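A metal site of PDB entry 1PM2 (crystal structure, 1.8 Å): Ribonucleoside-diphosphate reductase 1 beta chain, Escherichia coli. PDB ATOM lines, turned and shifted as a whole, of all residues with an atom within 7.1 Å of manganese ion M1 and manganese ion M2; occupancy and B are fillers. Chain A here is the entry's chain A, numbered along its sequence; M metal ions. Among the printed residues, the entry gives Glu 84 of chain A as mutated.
CZ of Phe 208 touches manganese ion M2, at 3.7 Å.
Of the 25 residues printed, 5 come within 4 Å of manganese ion M2.
Along chain A the residues within 4 Å of manganese ion M2 span positions 84 to 238.
The nearest printed residue that does not touch manganese ion M2 is Ile 234 (4.1 Å).
Manganese ion M2 is bound by OE1 of Glu 238 (1.9 Å), ND1 of His 118 (2.0 Å), OE1 of Glu 115 (2.1 Å), OE2 of Glu 84 (2.2 Å) and OE1 of Glu 84 (2.3 Å).
Manganese ion M2 has five donor atoms within binding distance.
The indole nitrogen of Trp 111 sits at hydrogen-bond distance from the side-chain carboxylate of Glu 204.
A ring nitrogen (NE2) of His 241 sits close to the backbone carbonyl oxygen of Asp 237, at 3.5 Å.
The backbone carbonyl oxygen (O) of Trp 111 lies within hydrogen-bond range of the side-chain hydroxyl (OG) of Ser 114 (2.6 Å).
O of Glu 115 sits at hydrogen-bond distance from OG of Ser 119 (3.4 Å).
A ring nitrogen (NE2) of His 118 sits close to the backbone carbonyl oxygen (O) of Ser 114, at 3.4 Å.
OE2 of Glu 115 lies close to NE1 of Trp 111 (3.2 Å).
NE2 of His 241 sits at hydrogen-bond distance from OG of Ser 114 (2.8 Å).
The backbone carbonyl oxygen (O) of Glu 84 is in hydrogen-bond range of the side-chain hydroxyl (OG) of Ser 119, at 3.3 Å.
OE2 of Glu 238 is bound to manganese ion M1, 2.0 Å away.
ND1 of His 241 binds manganese ion M1 (2.0 Å).
The side-chain carboxylate (OE2) of Glu 115 binds manganese ion M1 (2.1 Å).
Manganese ion M1 is bound by OE1 of Glu 204, 2.1 Å away.
Slightly farther from manganese ion M1 lies OE2 of Glu 204 (2.9 Å).
Trp 111 touches manganese ion M1.
Phe 208 touches manganese ion M1.
Within 4 Å of manganese ion M1: Trp 111, Glu 115, Glu 204, Phe 208, Glu 238 and His 241.
The nearest printed residue that does not touch manganese ion M1 is His 118 (4.9 Å).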
ATOM      1  N   GLN A  43      15.200  -4.675   0.868  1.00  0.00           N
ATOM      2  CA  GLN A  43      14.595  -3.910  -0.217  1.00  0.00           C
ATOM      3  C   GLN A  43      15.092  -4.409  -1.575  1.00  0.00           C
ATOM      4  O   GLN A  43      14.318  -4.509  -2.526  1.00  0.00           O
ATOM      5  CB  GLN A  43      14.889  -2.410  -0.052  1.00  0.00           C
ATOM      6  CG  GLN A  43      14.188  -1.523  -1.072  1.00  0.00           C
ATOM      7  CD  GLN A  43      12.667  -1.589  -0.989  1.00  0.00           C
ATOM      8  OE1 GLN A  43      12.041  -0.848  -0.228  1.00  0.00           O
ATOM      9  NE2 GLN A  43      12.068  -2.477  -1.779  1.00  0.00           N
ATOM     10  N   GLN A  80      -2.235   8.680  -3.820  1.00  0.00           N
ATOM     11  CA  GLN A  80      -1.105   7.777  -3.694  1.00  0.00           C
ATOM     12  C   GLN A  80       0.006   8.254  -4.643  1.00  0.00           C
ATOM     13  O   GLN A  80       1.180   8.256  -4.278  1.00  0.00           O
ATOM     14  CB  GLN A  80      -1.522   6.345  -4.066  1.00  0.00           C
ATOM     15  CG  GLN A  80      -2.579   5.727  -3.143  1.00  0.00           C
ATOM     16  CD  GLN A  80      -3.033   4.347  -3.585  1.00  0.00           C
ATOM     17  OE1 GLN A  80      -3.301   4.111  -4.769  1.00  0.00           O
ATOM     18  NE2 GLN A  80      -3.136   3.425  -2.634  1.00  0.00           N
ATOM     19  N   LEU A  83       1.815  11.297  -3.213  1.00  0.00           N
ATOM     20  CA  LEU A  83       2.754  10.904  -2.171  1.00  0.00           C
ATOM     21  C   LEU A  83       4.018  10.244  -2.713  1.00  0.00           C
ATOM     22  O   LEU A  83       5.106  10.490  -2.198  1.00  0.00           O
ATOM     23  CB  LEU A  83       2.082   9.978  -1.163  1.00  0.00           C
ATOM     24  CG  LEU A  83       0.992  10.585  -0.266  1.00  0.00           C
ATOM     25  CD1 LEU A  83       0.585   9.559   0.782  1.00  0.00           C
ATOM     26  CD2 LEU A  83       1.501  11.853   0.402  1.00  0.00           C
ATOM     27  N   GLU A  84       3.883   9.417  -3.729  1.00  0.00           N
ATOM     28  CA  GLU A  84       5.043   8.746  -4.313  1.00  0.00           C
ATOM     29  C   GLU A  84       5.936   9.742  -5.065  1.00  0.00           C
ATOM     30  O   GLU A  84       7.156   9.618  -5.077  1.00  0.00           O
ATOM     31  CB  GLU A  84       4.615   7.605  -5.237  1.00  0.00           C
ATOM     32  CG  GLU A  84       3.805   6.522  -4.532  1.00  0.00           C
ATOM     33  CD  GLU A  84       4.630   5.694  -3.554  1.00  0.00           C
ATOM     34  OE1 GLU A  84       5.767   6.092  -3.234  1.00  0.00           O
ATOM     35  OE2 GLU A  84       4.126   4.644  -3.108  1.00  0.00           O
ATOM     36  N   GLN A  87       7.806  11.369  -2.314  1.00  0.00           N
ATOM     37  CA  GLN A  87       8.723  10.429  -1.672  1.00  0.00           C
ATOM     38  C   GLN A  87       9.836   9.921  -2.566  1.00  0.00           C
ATOM     39  O   GLN A  87      10.831   9.390  -2.077  1.00  0.00           O
ATOM     40  CB  GLN A  87       7.946   9.254  -1.077  1.00  0.00           C
ATOM     41  CG  GLN A  87       7.184   9.599   0.199  1.00  0.00           C
ATOM     42  CD  GLN A  87       8.065  10.293   1.225  1.00  0.00           C
ATOM     43  OE1 GLN A  87       8.256  11.514   1.179  1.00  0.00           O
ATOM     44  NE2 GLN A  87       8.636   9.516   2.132  1.00  0.00           N
ATOM     45  N   TRP A 111      15.768   3.579  -0.553  1.00  0.00           N
ATOM     46  CA  TRP A 111      14.393   3.835  -0.158  1.00  0.00           C
ATOM     47  C   TRP A 111      13.770   4.775  -1.191  1.00  0.00           C
ATOM     48  O   TRP A 111      12.684   4.506  -1.725  1.00  0.00           O
ATOM     49  CB  TRP A 111      14.422   4.443   1.253  1.00  0.00           C
ATOM     50  CG  TRP A 111      13.209   5.186   1.729  1.00  0.00           C
ATOM     51  CD1 TRP A 111      11.921   5.087   1.268  1.00  0.00           C
ATOM     52  CD2 TRP A 111      13.167   6.106   2.827  1.00  0.00           C
ATOM     53  NE1 TRP A 111      11.093   5.893   2.008  1.00  0.00           N
ATOM     54  CE2 TRP A 111      11.838   6.530   2.976  1.00  0.00           C
ATOM     55  CE3 TRP A 111      14.147   6.614   3.696  1.00  0.00           C
ATOM     56  CZ2 TRP A 111      11.443   7.449   3.967  1.00  0.00           C
ATOM     57  CZ3 TRP A 111      13.757   7.521   4.681  1.00  0.00           C
ATOM     58  CH2 TRP A 111      12.409   7.925   4.804  1.00  0.00           C
ATOM     59  N   SER A 114      13.131   3.030  -4.517  1.00  0.00           N
ATOM     60  CA  SER A 114      11.943   2.176  -4.493  1.00  0.00           C
ATOM     61  C   SER A 114      10.665   2.997  -4.653  1.00  0.00           C
ATOM     62  O   SER A 114       9.675   2.517  -5.205  1.00  0.00           O
ATOM     63  CB  SER A 114      11.887   1.341  -3.217  1.00  0.00           C
ATOM     64  OG  SER A 114      11.597   2.138  -2.077  1.00  0.00           O
ATOM     65  N   GLU A 115      10.674   4.248  -4.176  1.00  0.00           N
ATOM     66  CA  GLU A 115       9.503   5.100  -4.296  1.00  0.00           C
ATOM     67  C   GLU A 115       9.303   5.498  -5.765  1.00  0.00           C
ATOM     68  O   GLU A 115       8.166   5.643  -6.217  1.00  0.00           O
ATOM     69  CB  GLU A 115       9.647   6.354  -3.420  1.00  0.00           C
ATOM     70  CG  GLU A 115       9.943   6.058  -1.949  1.00  0.00           C
ATOM     71  CD  GLU A 115       8.729   5.553  -1.182  1.00  0.00           C
ATOM     72  OE1 GLU A 115       7.937   4.768  -1.734  1.00  0.00           O
ATOM     73  OE2 GLU A 115       8.588   5.937   0.005  1.00  0.00           O
ATOM     74  N   THR A 116      10.389   5.673  -6.516  1.00  0.00           N
ATOM     75  CA  THR A 116      10.240   6.045  -7.925  1.00  0.00           C
ATOM     76  C   THR A 116       9.650   4.859  -8.673  1.00  0.00           C
ATOM     77  O   THR A 116       8.950   5.035  -9.677  1.00  0.00           O
ATOM     78  CB  THR A 116      11.578   6.438  -8.600  1.00  0.00           C
ATOM     79  OG1 THR A 116      12.449   5.303  -8.683  1.00  0.00           O
ATOM     80  CG2 THR A 116      12.252   7.555  -7.829  1.00  0.00           C
ATOM     81  N   ILE A 117       9.929   3.648  -8.201  1.00  0.00           N
ATOM     82  CA  ILE A 117       9.364   2.458  -8.835  1.00  0.00           C
ATOM     83  C   ILE A 117       7.864   2.471  -8.569  1.00  0.00           C
ATOM     84  O   ILE A 117       7.060   2.128  -9.435  1.00  0.00           O
ATOM     85  CB  ILE A 117       9.982   1.157  -8.266  1.00  0.00           C
ATOM     86  CG1 ILE A 117      11.460   1.062  -8.673  1.00  0.00           C
ATOM     87  CG2 ILE A 117       9.218  -0.065  -8.783  1.00  0.00           C
ATOM     88  CD1 ILE A 117      11.693   0.971 -10.178  1.00  0.00           C
ATOM     89  N   HIS A 118       7.496   2.881  -7.356  1.00  0.00           N
ATOM     90  CA  HIS A 118       6.076   2.967  -7.006  1.00  0.00           C
ATOM     91  C   HIS A 118       5.399   3.973  -7.926  1.00  0.00           C
ATOM     92  O   HIS A 118       4.290   3.735  -8.420  1.00  0.00           O
ATOM     93  CB  HIS A 118       5.921   3.386  -5.538  1.00  0.00           C
ATOM     94  CG  HIS A 118       6.451   2.380  -4.561  1.00  0.00           C
ATOM     95  ND1 HIS A 118       6.432   2.589  -3.205  1.00  0.00           N
ATOM     96  CD2 HIS A 118       7.015   1.160  -4.749  1.00  0.00           C
ATOM     97  CE1 HIS A 118       6.965   1.551  -2.595  1.00  0.00           C
ATOM     98  NE2 HIS A 118       7.330   0.668  -3.511  1.00  0.00           N
ATOM     99  N   SER A 119       6.061   5.103  -8.167  1.00  0.00           N
ATOM    100  CA  SER A 119       5.513   6.134  -9.053  1.00  0.00           C
ATOM    101  C   SER A 119       5.326   5.534 -10.452  1.00  0.00           C
ATOM    102  O   SER A 119       4.319   5.780 -11.115  1.00  0.00           O
ATOM    103  CB  SER A 119       6.457   7.337  -9.153  1.00  0.00           C
ATOM    104  OG  SER A 119       6.514   8.042  -7.923  1.00  0.00           O
ATOM    105  N   TYR A 122       2.241   3.449 -10.740  1.00  0.00           N
ATOM    106  CA  TYR A 122       0.985   4.189 -10.847  1.00  0.00           C
ATOM    107  C   TYR A 122       0.760   4.702 -12.265  1.00  0.00           C
ATOM    108  O   TYR A 122      -0.382   4.796 -12.719  1.00  0.00           O
ATOM    109  CB  TYR A 122       0.945   5.327  -9.824  1.00  0.00           C
ATOM    110  CG  TYR A 122       0.643   4.822  -8.429  1.00  0.00           C
ATOM    111  CD1 TYR A 122      -0.503   4.077  -8.183  1.00  0.00           C
ATOM    112  CD2 TYR A 122       1.517   5.057  -7.365  1.00  0.00           C
ATOM    113  CE1 TYR A 122      -0.787   3.574  -6.916  1.00  0.00           C
ATOM    114  CE2 TYR A 122       1.248   4.552  -6.084  1.00  0.00           C
ATOM    115  CZ  TYR A 122       0.089   3.816  -5.868  1.00  0.00           C
ATOM    116  OH  TYR A 122      -0.187   3.310  -4.622  1.00  0.00           O
ATOM    117  N   LEU A 203       3.671   9.697   7.348  1.00  0.00           N
ATOM    118  CA  LEU A 203       3.330   9.587   5.929  1.00  0.00           C
ATOM    119  C   LEU A 203       3.419   8.111   5.499  1.00  0.00           C
ATOM    120  O   LEU A 203       2.478   7.557   4.949  1.00  0.00           O
ATOM    121  CB  LEU A 203       4.294  10.443   5.094  1.00  0.00           C
ATOM    122  CG  LEU A 203       4.053  10.597   3.581  1.00  0.00           C
ATOM    123  CD1 LEU A 203       4.952  11.711   3.058  1.00  0.00           C
ATOM    124  CD2 LEU A 203       4.345   9.297   2.840  1.00  0.00           C
ATOM    125  N   GLU A 204       4.562   7.503   5.798  1.00  0.00           N
ATOM    126  CA  GLU A 204       4.819   6.099   5.439  1.00  0.00           C
ATOM    127  C   GLU A 204       3.931   5.089   6.171  1.00  0.00           C
ATOM    128  O   GLU A 204       3.399   4.164   5.564  1.00  0.00           O
ATOM    129  CB  GLU A 204       6.285   5.757   5.751  1.00  0.00           C
ATOM    130  CG  GLU A 204       7.354   6.581   5.033  1.00  0.00           C
ATOM    131  CD  GLU A 204       7.607   6.122   3.605  1.00  0.00           C
ATOM    132  OE1 GLU A 204       7.173   4.996   3.255  1.00  0.00           O
ATOM    133  OE2 GLU A 204       8.245   6.866   2.831  1.00  0.00           O
ATOM    134  N   PHE A 208      -0.113   6.208   3.788  1.00  0.00           N
ATOM    135  CA  PHE A 208      -0.069   5.152   2.769  1.00  0.00           C
ATOM    136  C   PHE A 208      -1.036   4.001   3.090  1.00  0.00           C
ATOM    137  O   PHE A 208      -1.734   3.517   2.205  1.00  0.00           O
ATOM    138  CB  PHE A 208       1.348   4.573   2.617  1.00  0.00           C
ATOM    139  CG  PHE A 208       2.220   5.333   1.650  1.00  0.00           C
ATOM    140  CD1 PHE A 208       1.722   5.723   0.409  1.00  0.00           C
ATOM    141  CD2 PHE A 208       3.536   5.626   1.967  1.00  0.00           C
ATOM    142  CE1 PHE A 208       2.544   6.397  -0.506  1.00  0.00           C
ATOM    143  CE2 PHE A 208       4.365   6.300   1.060  1.00  0.00           C
ATOM    144  CZ  PHE A 208       3.857   6.681  -0.187  1.00  0.00           C
ATOM    145  N   PHE A 212      -4.158   2.157   1.202  1.00  0.00           N
ATOM    146  CA  PHE A 212      -4.148   0.748   0.828  1.00  0.00           C
ATOM    147  C   PHE A 212      -5.511   0.141   1.116  1.00  0.00           C
ATOM    148  O   PHE A 212      -6.022  -0.655   0.323  1.00  0.00           O
ATOM    149  CB  PHE A 212      -3.073  -0.029   1.602  1.00  0.00           C
ATOM    150  CG  PHE A 212      -1.662   0.414   1.333  1.00  0.00           C
ATOM    151  CD1 PHE A 212      -1.326   1.060   0.158  1.00  0.00           C
ATOM    152  CD2 PHE A 212      -0.656   0.170   2.274  1.00  0.00           C
ATOM    153  CE1 PHE A 212      -0.018   1.466  -0.100  1.00  0.00           C
ATOM    154  CE2 PHE A 212       0.649   0.568   2.032  1.00  0.00           C
ATOM    155  CZ  PHE A 212       0.978   1.214   0.849  1.00  0.00           C
ATOM    156  N   ILE A 234       3.752  -2.690  -3.293  1.00  0.00           N
ATOM    157  CA  ILE A 234       4.089  -1.392  -2.721  1.00  0.00           C
ATOM    158  C   ILE A 234       4.052  -1.459  -1.197  1.00  0.00           C
ATOM    159  O   ILE A 234       4.966  -0.978  -0.518  1.00  0.00           O
ATOM    160  CB  ILE A 234       3.102  -0.293  -3.196  1.00  0.00           C
ATOM    161  CG1 ILE A 234       3.332  -0.020  -4.686  1.00  0.00           C
ATOM    162  CG2 ILE A 234       3.304   0.983  -2.373  1.00  0.00           C
ATOM    163  CD1 ILE A 234       2.397   1.044  -5.271  1.00  0.00           C
ATOM    164  N   ALA A 235       2.997  -2.058  -0.647  1.00  0.00           N
ATOM    165  CA  ALA A 235       2.848  -2.179   0.797  1.00  0.00           C
ATOM    166  C   ALA A 235       4.015  -2.954   1.413  1.00  0.00           C
ATOM    167  O   ALA A 235       4.456  -2.644   2.510  1.00  0.00           O
ATOM    168  CB  ALA A 235       1.522  -2.872   1.136  1.00  0.00           C
ATOM    169  N   ASP A 237       6.997  -2.903   0.409  1.00  0.00           N
ATOM    170  CA  ASP A 237       8.109  -1.963   0.440  1.00  0.00           C
ATOM    171  C   ASP A 237       7.906  -0.923   1.538  1.00  0.00           C
ATOM    172  O   ASP A 237       8.824  -0.601   2.279  1.00  0.00           O
ATOM    173  CB  ASP A 237       8.252  -1.229  -0.903  1.00  0.00           C
ATOM    174  CG  ASP A 237       8.705  -2.135  -2.030  1.00  0.00           C
ATOM    175  OD1 ASP A 237       9.359  -3.158  -1.756  1.00  0.00           O
ATOM    176  OD2 ASP A 237       8.417  -1.797  -3.201  1.00  0.00           O
ATOM    177  N   GLU A 238       6.682  -0.395   1.640  1.00  0.00           N
ATOM    178  CA  GLU A 238       6.377   0.598   2.651  1.00  0.00           C
ATOM    179  C   GLU A 238       6.643   0.074   4.056  1.00  0.00           C
ATOM    180  O   GLU A 238       7.036   0.837   4.945  1.00  0.00           O
ATOM    181  CB  GLU A 238       4.913   1.065   2.531  1.00  0.00           C
ATOM    182  CG  GLU A 238       4.549   1.616   1.165  1.00  0.00           C
ATOM    183  CD  GLU A 238       5.430   2.786   0.735  1.00  0.00           C
ATOM    184  OE1 GLU A 238       5.314   3.208  -0.437  1.00  0.00           O
ATOM    185  OE2 GLU A 238       6.210   3.305   1.560  1.00  0.00           O
ATOM    186  N   ALA A 239       6.443  -1.231   4.254  1.00  0.00           N
ATOM    187  CA  ALA A 239       6.687  -1.833   5.561  1.00  0.00           C
ATOM    188  C   ALA A 239       8.156  -1.651   5.941  1.00  0.00           C
ATOM    189  O   ALA A 239       8.489  -1.391   7.108  1.00  0.00           O
ATOM    190  CB  ALA A 239       6.342  -3.316   5.529  1.00  0.00           C
ATOM    191  N   LEU A 240       9.037  -1.794   4.963  1.00  0.00           N
ATOM    192  CA  LEU A 240      10.466  -1.619   5.202  1.00  0.00           C
ATOM    193  C   LEU A 240      10.775  -0.161   5.485  1.00  0.00           C
ATOM    194  O   LEU A 240      11.588   0.159   6.354  1.00  0.00           O
ATOM    195  CB  LEU A 240      11.292  -2.056   3.979  1.00  0.00           C
ATOM    196  CG  LEU A 240      11.246  -3.519   3.554  1.00  0.00           C
ATOM    197  CD1 LEU A 240      12.118  -3.700   2.317  1.00  0.00           C
ATOM    198  CD2 LEU A 240      11.734  -4.405   4.695  1.00  0.00           C
ATOM    199  N   HIS A 241      10.147   0.729   4.728  1.00  0.00           N
ATOM    200  CA  HIS A 241      10.358   2.154   4.879  1.00  0.00           C
ATOM    201  C   HIS A 241       9.993   2.655   6.266  1.00  0.00           C
ATOM    202  O   HIS A 241      10.762   3.383   6.904  1.00  0.00           O
ATOM    203  CB  HIS A 241       9.558   2.927   3.829  1.00  0.00           C
ATOM    204  CG  HIS A 241       9.901   2.542   2.422  1.00  0.00           C
ATOM    205  ND1 HIS A 241       9.205   3.007   1.336  1.00  0.00           N
ATOM    206  CD2 HIS A 241      10.875   1.739   1.931  1.00  0.00           C
ATOM    207  CE1 HIS A 241       9.730   2.509   0.226  1.00  0.00           C
ATOM    208  NE2 HIS A 241      10.738   1.731   0.566  1.00  0.00           N
ATOM    209  N   LEU A 242       8.825   2.254   6.765  1.00  0.00           N
ATOM    210  CA  LEU A 242       8.407   2.709   8.086  1.00  0.00           C
ATOM    211  C   LEU A 242       9.262   2.050   9.166  1.00  0.00           C
ATOM    212  O   LEU A 242       9.456   2.611  10.234  1.00  0.00           O
ATOM    213  CB  LEU A 242       6.916   2.444   8.299  1.00  0.00           C
ATOM    214  CG  LEU A 242       6.378   1.025   8.431  1.00  0.00           C
ATOM    215  CD1 LEU A 242       6.528   0.563   9.871  1.00  0.00           C
ATOM    216  CD2 LEU A 242       4.908   0.994   8.012  1.00  0.00           C
HETATM  217 MN    MN M   1       7.817   4.469   1.310  1.00  0.00          MN
HETATM  218 MN    MN M   2       5.921   4.159  -2.003  1.00  0.00          MN
